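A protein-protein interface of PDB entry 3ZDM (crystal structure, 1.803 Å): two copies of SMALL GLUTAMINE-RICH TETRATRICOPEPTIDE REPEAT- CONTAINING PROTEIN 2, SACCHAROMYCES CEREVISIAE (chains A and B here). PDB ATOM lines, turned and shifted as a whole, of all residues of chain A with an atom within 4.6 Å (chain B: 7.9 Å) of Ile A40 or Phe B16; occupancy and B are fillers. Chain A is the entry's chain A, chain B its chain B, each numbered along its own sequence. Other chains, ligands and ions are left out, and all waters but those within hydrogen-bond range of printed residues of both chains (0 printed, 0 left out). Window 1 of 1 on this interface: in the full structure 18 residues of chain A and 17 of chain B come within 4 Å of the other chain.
The backbone carbonyl oxygen of Ser B32 lies close to the side-chain sulfur of Cys A39 (3.5 Å).
Among the printed residues, merely in contact across the chains: Ile A12 with Ile B12, Ile A12 with Phe B16, Phe A16 with Ile B12, Phe A16 with Ile B40, Ala A36 with Ala B36, Ala A36 with Ile B40, Cys A39 with Val B35, Cys A39 with Ala B36, Ile A40 with Phe B16, Glu A42 with Ser B32, Ala A43 with Ile B25, Ala A43 with Gly B29, Ala A43 with Leu B33, Phe A44 with Phe B16 and Phe A44 with Leu B33.
Of chain B, only Phe B16 comes within 4 Å of Ile A40. Phe B16 touches just these residues of chain A: Ile A12 (3.6 Å), Ile A40 (3.6 Å) and Phe A44 (3.7 Å). Ile B19 touches none of the printed residues of chain A. Printed residues of chain A within 4 Å of Ser B32: Cys A39 and Glu A42. Asn B34 touches none of the printed residues of chain A. Printed residues of chain A within 4 Å of Ile B40: Phe A16 (3.6 Å) and Ala A36 (3.97 Å). The nearest printed residue of chain B that does not touch Ile A40 is Ala B36 (4.1 Å). The nearest printed residue of chain A that does not touch Phe B16 is Ala A9 (5.0 Å).
Of the 13 printed residues of chain A, 8 touch a printed residue of chain B. Hydrophobic or aromatic side chains of chain A that line the printed part of chain B: Ile A12, Phe A16, Ala A36, Ile A40, Ala A43 and Phe A44. Hydrophobic or aromatic side chains of chain B that line the printed part of chain A: Ile B12, Phe B16, Ile B25, Leu B33, Val B35, Ala B36 and Ile B40. Among the printed residues, 16 pairs touch across the chains.
Ile A12 touches its own counterpart, Ile B12. Ile A12 touches Phe B16, and with the chains exchanged Phe A16 touches Ile B12. Phe A16 touches Ile B40, and with the chains exchanged Ile A40 touches Phe B16. Ala A36 touches Ile B40, but with the chains exchanged Ile A40 does not touch Ala B36 (4.1 Å). Positions printed for both chains: 9, 12, 13, 16, 36, 37 and 40. Of the 16 pairs that touch across the chains among the printed residues, 6 have their exchanged pair printed and touching as well.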
ATOM      1  N   ALA A   9       8.310   2.415  -7.453  1.00  0.00           N
ATOM      2  CA  ALA A   9       8.726   1.172  -8.042  1.00  0.00           C
ATOM      3  C   ALA A   9       8.115   0.962  -9.416  1.00  0.00           C
ATOM      4  O   ALA A   9       8.779   0.493 -10.316  1.00  0.00           O
ATOM      5  CB  ALA A   9       8.337  -0.038  -7.119  1.00  0.00           C
ATOM      6  N   ILE A  12       9.914   3.069 -11.901  1.00  0.00           N
ATOM      7  CA  ILE A  12      11.230   2.522 -12.222  1.00  0.00           C
ATOM      8  C   ILE A  12      11.064   1.357 -13.206  1.00  0.00           C
ATOM      9  O   ILE A  12      11.802   1.247 -14.186  1.00  0.00           O
ATOM     10  CB  ILE A  12      11.957   2.066 -10.938  1.00  0.00           C
ATOM     11  CG1 ILE A  12      12.211   3.290 -10.035  1.00  0.00           C
ATOM     12  CG2 ILE A  12      13.221   1.177 -11.237  1.00  0.00           C
ATOM     13  CD1 ILE A  12      12.727   2.903  -8.615  1.00  0.00           C
ATOM     14  N   VAL A  13      10.086   0.494 -12.948  1.00  0.00           N
ATOM     15  CA  VAL A  13       9.829  -0.614 -13.866  1.00  0.00           C
ATOM     16  C   VAL A  13       9.444  -0.051 -15.255  1.00  0.00           C
ATOM     17  O   VAL A  13       9.909  -0.533 -16.291  1.00  0.00           O
ATOM     18  CB  VAL A  13       8.754  -1.542 -13.318  1.00  0.00           C
ATOM     19  CG1 VAL A  13       8.256  -2.517 -14.403  1.00  0.00           C
ATOM     20  CG2 VAL A  13       9.327  -2.339 -12.092  1.00  0.00           C
ATOM     21  N   PHE A  16      12.626   1.133 -17.127  1.00  0.00           N
ATOM     22  CA  PHE A  16      13.389   0.021 -17.687  1.00  0.00           C
ATOM     23  C   PHE A  16      12.615  -0.631 -18.824  1.00  0.00           C
ATOM     24  O   PHE A  16      13.182  -1.115 -19.798  1.00  0.00           O
ATOM     25  CB  PHE A  16      13.612  -1.039 -16.587  1.00  0.00           C
ATOM     26  CG  PHE A  16      14.577  -0.610 -15.484  1.00  0.00           C
ATOM     27  CD1 PHE A  16      15.440   0.459 -15.676  1.00  0.00           C
ATOM     28  CD2 PHE A  16      14.610  -1.301 -14.260  1.00  0.00           C
ATOM     29  CE1 PHE A  16      16.354   0.852 -14.674  1.00  0.00           C
ATOM     30  CE2 PHE A  16      15.487  -0.909 -13.236  1.00  0.00           C
ATOM     31  CZ  PHE A  16      16.375   0.136 -13.436  1.00  0.00           C
ATOM     32  N   ALA A  36      15.614  -7.745 -13.386  1.00  0.00           N
ATOM     33  CA  ALA A  36      15.444  -6.633 -12.438  1.00  0.00           C
ATOM     34  C   ALA A  36      13.960  -6.239 -12.347  1.00  0.00           C
ATOM     35  O   ALA A  36      13.449  -6.038 -11.255  1.00  0.00           O
ATOM     36  CB  ALA A  36      16.293  -5.406 -12.883  1.00  0.00           C
ATOM     37  N   MET A  37      13.273  -6.130 -13.490  1.00  0.00           N
ATOM     38  CA  MET A  37      11.820  -5.755 -13.464  1.00  0.00           C
ATOM     39  C   MET A  37      10.984  -6.807 -12.717  1.00  0.00           C
ATOM     40  O   MET A  37      10.105  -6.462 -11.925  1.00  0.00           O
ATOM     41  CB  MET A  37      11.263  -5.459 -14.839  1.00  0.00           C
ATOM     42  CG  MET A  37      11.881  -4.214 -15.444  1.00  0.00           C
ATOM     43  SD  MET A  37      11.080  -3.791 -17.018  1.00  0.00           S
ATOM     44  CE  MET A  37      12.100  -4.701 -18.153  1.00  0.00           C
ATOM     45  N   ASP A  38      11.249  -8.085 -12.966  1.00  0.00           N
ATOM     46  CA  ASP A  38      10.521  -9.107 -12.225  1.00  0.00           C
ATOM     47  C   ASP A  38      10.792  -9.017 -10.721  1.00  0.00           C
ATOM     48  O   ASP A  38       9.861  -9.190  -9.929  1.00  0.00           O
ATOM     49  CB  ASP A  38      10.880 -10.520 -12.707  1.00  0.00           C
ATOM     50  CG  ASP A  38      10.275 -10.842 -14.044  1.00  0.00           C
ATOM     51  OD1 ASP A  38       9.362 -10.093 -14.502  1.00  0.00           O
ATOM     52  OD2 ASP A  38      10.717 -11.832 -14.638  1.00  0.00           O
ATOM     53  N   CYS A  39      12.059  -8.834 -10.324  1.00  0.00           N
ATOM     54  CA  CYS A  39      12.420  -8.701  -8.901  1.00  0.00           C
ATOM     55  C   CYS A  39      11.738  -7.492  -8.233  1.00  0.00           C
ATOM     56  O   CYS A  39      11.278  -7.572  -7.116  1.00  0.00           O
ATOM     57  CB  CYS A  39      13.915  -8.578  -8.709  1.00  0.00           C
ATOM     58  SG  CYS A  39      14.851 -10.085  -9.111  1.00  0.00           S
ATOM     59  N   ILE A  40      11.685  -6.365  -8.929  1.00  0.00           N
ATOM     60  CA  ILE A  40      11.065  -5.193  -8.340  1.00  0.00           C
ATOM     61  C   ILE A  40       9.576  -5.420  -8.140  1.00  0.00           C
ATOM     62  O   ILE A  40       9.018  -5.088  -7.079  1.00  0.00           O
ATOM     63  CB  ILE A  40      11.323  -3.973  -9.233  1.00  0.00           C
ATOM     64  CG1 ILE A  40      12.810  -3.668  -9.260  1.00  0.00           C
ATOM     65  CG2 ILE A  40      10.547  -2.784  -8.713  1.00  0.00           C
ATOM     66  CD1 ILE A  40      13.222  -2.678 -10.416  1.00  0.00           C
ATOM     67  N   SER A  41       8.941  -5.980  -9.173  1.00  0.00           N
ATOM     68  CA  SER A  41       7.525  -6.277  -9.154  1.00  0.00           C
ATOM     69  C   SER A  41       7.193  -7.229  -8.016  1.00  0.00           C
ATOM     70  O   SER A  41       6.213  -7.056  -7.288  1.00  0.00           O
ATOM     71  CB  SER A  41       7.087  -6.896 -10.485  1.00  0.00           C
ATOM     72  OG  SER A  41       7.296  -5.928 -11.512  1.00  0.00           O
ATOM     73  N   GLU A  42       8.026  -8.256  -7.877  1.00  0.00           N
ATOM     74  CA  GLU A  42       7.852  -9.201  -6.802  1.00  0.00           C
ATOM     75  C   GLU A  42       7.997  -8.517  -5.456  1.00  0.00           C
ATOM     76  O   GLU A  42       7.163  -8.733  -4.575  1.00  0.00           O
ATOM     77  CB  GLU A  42       8.862 -10.328  -6.936  1.00  0.00           C
ATOM     78  CG  GLU A  42       8.838 -11.313  -5.716  1.00  0.00           C
ATOM     79  CD  GLU A  42       7.829 -12.442  -5.807  1.00  0.00           C
ATOM     80  OE1 GLU A  42       7.241 -12.640  -6.879  1.00  0.00           O
ATOM     81  OE2 GLU A  42       7.665 -13.169  -4.800  1.00  0.00           O
ATOM     82  N   ALA A  43       9.011  -7.672  -5.327  1.00  0.00           N
ATOM     83  CA  ALA A  43       9.301  -7.022  -4.056  1.00  0.00           C
ATOM     84  C   ALA A  43       8.193  -6.101  -3.631  1.00  0.00           C
ATOM     85  O   ALA A  43       7.897  -6.028  -2.462  1.00  0.00           O
ATOM     86  CB  ALA A  43      10.604  -6.262  -4.104  1.00  0.00           C
ATOM     87  N   PHE A  44       7.564  -5.416  -4.575  1.00  0.00           N
ATOM     88  CA  PHE A  44       6.556  -4.421  -4.225  1.00  0.00           C
ATOM     89  C   PHE A  44       5.123  -4.906  -4.338  1.00  0.00           C
ATOM     90  O   PHE A  44       4.183  -4.172  -4.047  1.00  0.00           O
ATOM     91  CB  PHE A  44       6.809  -3.104  -5.019  1.00  0.00           C
ATOM     92  CG  PHE A  44       8.046  -2.358  -4.527  1.00  0.00           C
ATOM     93  CD1 PHE A  44       7.944  -1.463  -3.464  1.00  0.00           C
ATOM     94  CD2 PHE A  44       9.305  -2.606  -5.072  1.00  0.00           C
ATOM     95  CE1 PHE A  44       9.071  -0.804  -2.979  1.00  0.00           C
ATOM     96  CE2 PHE A  44      10.449  -1.936  -4.598  1.00  0.00           C
ATOM     97  CZ  PHE A  44      10.323  -1.022  -3.548  1.00  0.00           C
ATOM     98  N   ALA B   9      20.721   5.082 -12.939  1.00  0.00           N
ATOM     99  CA  ALA B   9      20.816   3.725 -12.396  1.00  0.00           C
ATOM    100  C   ALA B   9      21.343   3.755 -10.967  1.00  0.00           C
ATOM    101  O   ALA B   9      20.836   3.056 -10.109  1.00  0.00           O
ATOM    102  CB  ALA B   9      21.718   2.851 -13.257  1.00  0.00           C
ATOM    103  N   ALA B  10      22.353   4.579 -10.697  1.00  0.00           N
ATOM    104  CA  ALA B  10      22.869   4.664  -9.331  1.00  0.00           C
ATOM    105  C   ALA B  10      21.846   5.287  -8.357  1.00  0.00           C
ATOM    106  O   ALA B  10      21.770   4.876  -7.212  1.00  0.00           O
ATOM    107  CB  ALA B  10      24.188   5.392  -9.283  1.00  0.00           C
ATOM    108  N   LEU B  11      21.060   6.275  -8.787  1.00  0.00           N
ATOM    109  CA  LEU B  11      19.967   6.764  -7.907  1.00  0.00           C
ATOM    110  C   LEU B  11      18.891   5.719  -7.588  1.00  0.00           C
ATOM    111  O   LEU B  11      18.270   5.725  -6.508  1.00  0.00           O
ATOM    112  CB  LEU B  11      19.286   7.960  -8.547  1.00  0.00           C
ATOM    113  CG  LEU B  11      20.144   9.218  -8.585  1.00  0.00           C
ATOM    114  CD1 LEU B  11      19.505  10.270  -9.512  1.00  0.00           C
ATOM    115  CD2 LEU B  11      20.346   9.815  -7.177  1.00  0.00           C
ATOM    116  N   ILE B  12      18.664   4.827  -8.546  1.00  0.00           N
ATOM    117  CA  ILE B  12      17.682   3.789  -8.377  1.00  0.00           C
ATOM    118  C   ILE B  12      18.246   2.822  -7.369  1.00  0.00           C
ATOM    119  O   ILE B  12      17.577   2.425  -6.425  1.00  0.00           O
ATOM    120  CB  ILE B  12      17.340   3.090  -9.727  1.00  0.00           C
ATOM    121  CG1 ILE B  12      16.459   4.043 -10.571  1.00  0.00           C
ATOM    122  CG2 ILE B  12      16.649   1.745  -9.511  1.00  0.00           C
ATOM    123  CD1 ILE B  12      16.284   3.620 -12.071  1.00  0.00           C
ATOM    124  N   VAL B  13      19.498   2.452  -7.562  1.00  0.00           N
ATOM    125  CA  VAL B  13      20.122   1.508  -6.616  1.00  0.00           C
ATOM    126  C   VAL B  13      20.132   2.067  -5.182  1.00  0.00           C
ATOM    127  O   VAL B  13      19.908   1.344  -4.198  1.00  0.00           O
ATOM    128  CB  VAL B  13      21.561   1.115  -7.072  1.00  0.00           C
ATOM    129  CG1 VAL B  13      22.364   0.497  -5.950  1.00  0.00           C
ATOM    130  CG2 VAL B  13      21.493   0.160  -8.293  1.00  0.00           C
ATOM    131  N   ASN B  14      20.467   3.343  -5.070  1.00  0.00           N
ATOM    132  CA  ASN B  14      20.412   4.048  -3.788  1.00  0.00           C
ATOM    133  C   ASN B  14      19.005   4.037  -3.131  1.00  0.00           C
ATOM    134  O   ASN B  14      18.879   3.858  -1.912  1.00  0.00           O
ATOM    135  CB  ASN B  14      20.904   5.503  -3.978  1.00  0.00           C
ATOM    136  CG  ASN B  14      20.981   6.268  -2.664  1.00  0.00           C
ATOM    137  OD1 ASN B  14      21.954   6.149  -1.921  1.00  0.00           O
ATOM    138  ND2 ASN B  14      19.948   7.047  -2.370  1.00  0.00           N
ATOM    139  N   TYR B  15      17.962   4.244  -3.936  1.00  0.00           N
ATOM    140  CA  TYR B  15      16.587   4.224  -3.453  1.00  0.00           C
ATOM    141  C   TYR B  15      16.219   2.847  -2.892  1.00  0.00           C
ATOM    142  O   TYR B  15      15.667   2.722  -1.780  1.00  0.00           O
ATOM    143  CB  TYR B  15      15.614   4.610  -4.575  1.00  0.00           C
ATOM    144  CG  TYR B  15      14.166   4.514  -4.152  1.00  0.00           C
ATOM    145  CD1 TYR B  15      13.630   5.419  -3.259  1.00  0.00           C
ATOM    146  CD2 TYR B  15      13.346   3.519  -4.646  1.00  0.00           C
ATOM    147  CE1 TYR B  15      12.291   5.312  -2.850  1.00  0.00           C
ATOM    148  CE2 TYR B  15      12.032   3.391  -4.238  1.00  0.00           C
ATOM    149  CZ  TYR B  15      11.500   4.298  -3.347  1.00  0.00           C
ATOM    150  OH  TYR B  15      10.174   4.172  -2.953  1.00  0.00           O
ATOM    151  N   PHE B  16      16.486   1.811  -3.673  1.00  0.00           N
ATOM    152  CA  PHE B  16      16.235   0.439  -3.204  1.00  0.00           C
ATOM    153  C   PHE B  16      17.046   0.099  -1.960  1.00  0.00           C
ATOM    154  O   PHE B  16      16.567  -0.589  -1.064  1.00  0.00           O
ATOM    155  CB  PHE B  16      16.481  -0.597  -4.322  1.00  0.00           C
ATOM    156  CG  PHE B  16      15.461  -0.543  -5.433  1.00  0.00           C
ATOM    157  CD1 PHE B  16      14.183  -0.090  -5.182  1.00  0.00           C
ATOM    158  CD2 PHE B  16      15.801  -0.919  -6.755  1.00  0.00           C
ATOM    159  CE1 PHE B  16      13.202  -0.048  -6.201  1.00  0.00           C
ATOM    160  CE2 PHE B  16      14.851  -0.884  -7.778  1.00  0.00           C
ATOM    161  CZ  PHE B  16      13.529  -0.431  -7.501  1.00  0.00           C
ATOM    162  N   SER B  17      18.288   0.552  -1.897  1.00  0.00           N
ATOM    163  CA  SER B  17      19.115   0.247  -0.717  1.00  0.00           C
ATOM    164  C   SER B  17      18.496   0.826   0.583  1.00  0.00           C
ATOM    165  O   SER B  17      18.576   0.217   1.647  1.00  0.00           O
ATOM    166  CB  SER B  17      20.547   0.761  -0.880  1.00  0.00           C
ATOM    167  OG  SER B  17      21.188   0.151  -1.984  1.00  0.00           O
ATOM    168  N   SER B  18      17.883   1.997   0.482  1.00  0.00           N
ATOM    169  CA  SER B  18      17.230   2.640   1.628  1.00  0.00           C
ATOM    170  C   SER B  18      15.955   1.905   2.007  1.00  0.00           C
ATOM    171  O   SER B  18      15.616   1.805   3.188  1.00  0.00           O
ATOM    172  CB  SER B  18      16.892   4.105   1.286  1.00  0.00           C
ATOM    173  OG  SER B  18      15.903   4.146   0.270  1.00  0.00           O
ATOM    174  N   ILE B  19      15.237   1.382   1.014  1.00  0.00           N
ATOM    175  CA  ILE B  19      14.044   0.582   1.311  1.00  0.00           C
ATOM    176  C   ILE B  19      14.445  -0.681   2.061  1.00  0.00           C
ATOM    177  O   ILE B  19      13.808  -1.076   3.043  1.00  0.00           O
ATOM    178  CB  ILE B  19      13.274   0.214   0.012  1.00  0.00           C
ATOM    179  CG1 ILE B  19      12.690   1.479  -0.672  1.00  0.00           C
ATOM    180  CG2 ILE B  19      12.172  -0.796   0.297  1.00  0.00           C
ATOM    181  CD1 ILE B  19      11.423   1.970  -0.038  1.00  0.00           C
ATOM    182  N   VAL B  20      15.487  -1.348   1.590  1.00  0.00           N
ATOM    183  CA  VAL B  20      15.919  -2.542   2.290  1.00  0.00           C
ATOM    184  C   VAL B  20      16.445  -2.224   3.679  1.00  0.00           C
ATOM    185  O   VAL B  20      16.111  -2.895   4.667  1.00  0.00           O
ATOM    186  CB  VAL B  20      17.004  -3.309   1.481  1.00  0.00           C
ATOM    187  CG1 VAL B  20      17.701  -4.333   2.342  1.00  0.00           C
ATOM    188  CG2 VAL B  20      16.384  -3.953   0.251  1.00  0.00           C
ATOM    189  N   GLU B  21      17.296  -1.215   3.747  1.00  0.00           N
ATOM    190  CA  GLU B  21      17.962  -0.897   5.000  1.00  0.00           C
ATOM    191  C   GLU B  21      16.981  -0.474   6.074  1.00  0.00           C
ATOM    192  O   GLU B  21      17.239  -0.700   7.234  1.00  0.00           O
ATOM    193  CB  GLU B  21      19.087   0.137   4.789  1.00  0.00           C
ATOM    194  CG  GLU B  21      20.377  -0.486   4.212  1.00  0.00           C
ATOM    195  CD  GLU B  21      21.332   0.552   3.617  1.00  0.00           C
ATOM    196  OE1 GLU B  21      21.308   1.716   4.087  1.00  0.00           O
ATOM    197  OE2 GLU B  21      22.098   0.201   2.679  1.00  0.00           O
ATOM    198  N   LYS B  22      15.863   0.141   5.699  1.00  0.00           N
ATOM    199  CA  LYS B  22      14.873   0.529   6.695  1.00  0.00           C
ATOM    200  C   LYS B  22      13.810  -0.539   6.894  1.00  0.00           C
ATOM    201  O   LYS B  22      12.839  -0.321   7.616  1.00  0.00           O
ATOM    202  CB  LYS B  22      14.172   1.818   6.282  1.00  0.00           C
ATOM    203  CG  LYS B  22      15.078   3.022   6.130  1.00  0.00           C
ATOM    204  CD  LYS B  22      14.264   4.243   5.741  1.00  0.00           C
ATOM    205  CE  LYS B  22      15.120   5.299   5.062  1.00  0.00           C
ATOM    206  NZ  LYS B  22      15.353   6.472   5.950  1.00  0.00           N
ATOM    207  N   LYS B  23      13.984  -1.674   6.229  1.00  0.00           N
ATOM    208  CA  LYS B  23      13.061  -2.803   6.351  1.00  0.00           C
ATOM    209  C   LYS B  23      11.628  -2.437   6.000  1.00  0.00           C
ATOM    210  O   LYS B  23      10.707  -2.835   6.721  1.00  0.00           O
ATOM    211  CB  LYS B  23      13.075  -3.365   7.780  1.00  0.00           C
ATOM    212  CG  LYS B  23      14.440  -3.731   8.314  1.00  0.00           C
ATOM    213  CD  LYS B  23      14.323  -4.366   9.717  1.00  0.00           C
ATOM    214  CE  LYS B  23      15.659  -4.403  10.386  1.00  0.00           C
ATOM    215  NZ  LYS B  23      15.567  -4.968  11.778  1.00  0.00           N
ATOM    216  N   ILE B  25      10.061  -3.335   3.272  1.00  0.00           N
ATOM    217  CA  ILE B  25       9.424  -4.506   2.689  1.00  0.00           C
ATOM    218  C   ILE B  25      10.013  -5.749   3.396  1.00  0.00           C
ATOM    219  O   ILE B  25      10.966  -5.642   4.157  1.00  0.00           O
ATOM    220  CB  ILE B  25       9.642  -4.637   1.178  1.00  0.00           C
ATOM    221  CG1 ILE B  25      11.142  -4.665   0.863  1.00  0.00           C
ATOM    222  CG2 ILE B  25       8.908  -3.481   0.395  1.00  0.00           C
ATOM    223  CD1 ILE B  25      11.461  -4.952  -0.595  1.00  0.00           C
ATOM    224  N   GLY B  29      11.334  -9.809   0.033  1.00  0.00           N
ATOM    225  CA  GLY B  29      11.374  -8.631  -0.852  1.00  0.00           C
ATOM    226  C   GLY B  29      12.767  -8.068  -0.961  1.00  0.00           C
ATOM    227  O   GLY B  29      13.215  -7.674  -2.064  1.00  0.00           O
ATOM    228  N   ALA B  30      13.464  -8.005   0.181  1.00  0.00           N
ATOM    229  CA  ALA B  30      14.822  -7.490   0.143  1.00  0.00           C
ATOM    230  C   ALA B  30      15.763  -8.377  -0.676  1.00  0.00           C
ATOM    231  O   ALA B  30      16.601  -7.882  -1.442  1.00  0.00           O
ATOM    232  CB  ALA B  30      15.361  -7.226   1.538  1.00  0.00           C
ATOM    233  N   SER B  32      14.937 -10.034  -3.238  1.00  0.00           N
ATOM    234  CA  SER B  32      14.650  -9.750  -4.644  1.00  0.00           C
ATOM    235  C   SER B  32      15.245  -8.426  -5.082  1.00  0.00           C
ATOM    236  O   SER B  32      15.761  -8.311  -6.198  1.00  0.00           O
ATOM    237  CB  SER B  32      13.142  -9.737  -4.910  1.00  0.00           C
ATOM    238  OG  SER B  32      12.577 -11.023  -4.642  1.00  0.00           O
ATOM    239  N   LEU B  33      15.175  -7.419  -4.220  1.00  0.00           N
ATOM    240  CA  LEU B  33      15.744  -6.120  -4.559  1.00  0.00           C
ATOM    241  C   LEU B  33      17.268  -6.176  -4.650  1.00  0.00           C
ATOM    242  O   LEU B  33      17.880  -5.451  -5.459  1.00  0.00           O
ATOM    243  CB  LEU B  33      15.311  -5.046  -3.561  1.00  0.00           C
ATOM    244  CG  LEU B  33      13.882  -4.519  -3.725  1.00  0.00           C
ATOM    245  CD1 LEU B  33      13.659  -3.250  -2.844  1.00  0.00           C
ATOM    246  CD2 LEU B  33      13.550  -4.183  -5.229  1.00  0.00           C
ATOM    247  N   ASN B  34      17.891  -7.022  -3.840  1.00  0.00           N
ATOM    248  CA  ASN B  34      19.335  -7.126  -3.905  1.00  0.00           C
ATOM    249  C   ASN B  34      19.727  -7.687  -5.268  1.00  0.00           C
ATOM    250  O   ASN B  34      20.685  -7.227  -5.890  1.00  0.00           O
ATOM    251  CB  ASN B  34      19.911  -7.963  -2.743  1.00  0.00           C
ATOM    252  CG  ASN B  34      20.132  -7.135  -1.485  1.00  0.00           C
ATOM    253  OD1 ASN B  34      20.539  -5.982  -1.564  1.00  0.00           O
ATOM    254  ND2 ASN B  34      19.871  -7.730  -0.321  1.00  0.00           N
ATOM    255  N   VAL B  35      18.960  -8.661  -5.754  1.00  0.00           N
ATOM    256  CA  VAL B  35      19.246  -9.215  -7.089  1.00  0.00           C
ATOM    257  C   VAL B  35      19.001  -8.121  -8.153  1.00  0.00           C
ATOM    258  O   VAL B  35      19.810  -7.919  -9.071  1.00  0.00           O
ATOM    259  CB  VAL B  35      18.435 -10.475  -7.358  1.00  0.00           C
ATOM    260  CG1 VAL B  35      18.513 -10.906  -8.844  1.00  0.00           C
ATOM    261  CG2 VAL B  35      18.955 -11.662  -6.457  1.00  0.00           C
ATOM    262  N   ALA B  36      17.907  -7.391  -8.009  1.00  0.00           N
ATOM    263  CA  ALA B  36      17.625  -6.273  -8.934  1.00  0.00           C
ATOM    264  C   ALA B  36      18.778  -5.328  -9.070  1.00  0.00           C
ATOM    265  O   ALA B  36      19.164  -4.963 -10.186  1.00  0.00           O
ATOM    266  CB  ALA B  36      16.376  -5.489  -8.486  1.00  0.00           C
ATOM    267  N   MET B  37      19.309  -4.899  -7.927  1.00  0.00           N
ATOM    268  CA  MET B  37      20.406  -3.951  -7.907  1.00  0.00           C
ATOM    269  C   MET B  37      21.642  -4.461  -8.641  1.00  0.00           C
ATOM    270  O   MET B  37      22.294  -3.685  -9.388  1.00  0.00           O
ATOM    271  CB  MET B  37      20.716  -3.497  -6.477  1.00  0.00           C
ATOM    272  CG  MET B  37      19.527  -2.728  -5.851  1.00  0.00           C
ATOM    273  SD  MET B  37      19.938  -2.046  -4.254  1.00  0.00           S
ATOM    274  CE  MET B  37      19.151  -3.238  -3.216  1.00  0.00           C
ATOM    275  N   ILE B  40      20.830  -4.273 -12.329  1.00  0.00           N
ATOM    276  CA  ILE B  40      20.800  -2.884 -12.802  1.00  0.00           C
ATOM    277  C   ILE B  40      22.206  -2.385 -13.027  1.00  0.00           C
ATOM    278  O   ILE B  40      22.519  -1.771 -14.055  1.00  0.00           O
ATOM    279  CB  ILE B  40      20.017  -1.966 -11.799  1.00  0.00           C
ATOM    280  CG1 ILE B  40      18.525  -2.286 -11.871  1.00  0.00           C
ATOM    281  CG2 ILE B  40      20.257  -0.482 -12.111  1.00  0.00           C
ATOM    282  CD1 ILE B  40      17.750  -1.776 -10.611  1.00  0.00           C
ATOM    283  N   ARG B  48      28.082  -2.291  -8.353  1.00  0.00           N
ATOM    284  CA  ARG B  48      27.104  -1.804  -7.393  1.00  0.00           C
ATOM    285  C   ARG B  48      27.773  -1.049  -6.243  1.00  0.00           C
ATOM    286  O   ARG B  48      27.193  -0.140  -5.641  1.00  0.00           O
ATOM    287  CB  ARG B  48      26.279  -2.973  -6.856  1.00  0.00           C
ATOM    288  CG  ARG B  48      25.173  -2.571  -5.923  1.00  0.00           C
ATOM    289  CD  ARG B  48      24.203  -3.690  -5.809  1.00  0.00           C
ATOM    290  NE  ARG B  48      23.645  -3.783  -4.475  1.00  0.00           N
ATOM    291  CZ  ARG B  48      23.179  -4.911  -3.950  1.00  0.00           C
ATOM    292  NH1 ARG B  48      23.256  -6.065  -4.625  1.00  0.00           N
ATOM    293  NH2 ARG B  48      22.652  -4.888  -2.744  1.00  0.00           N
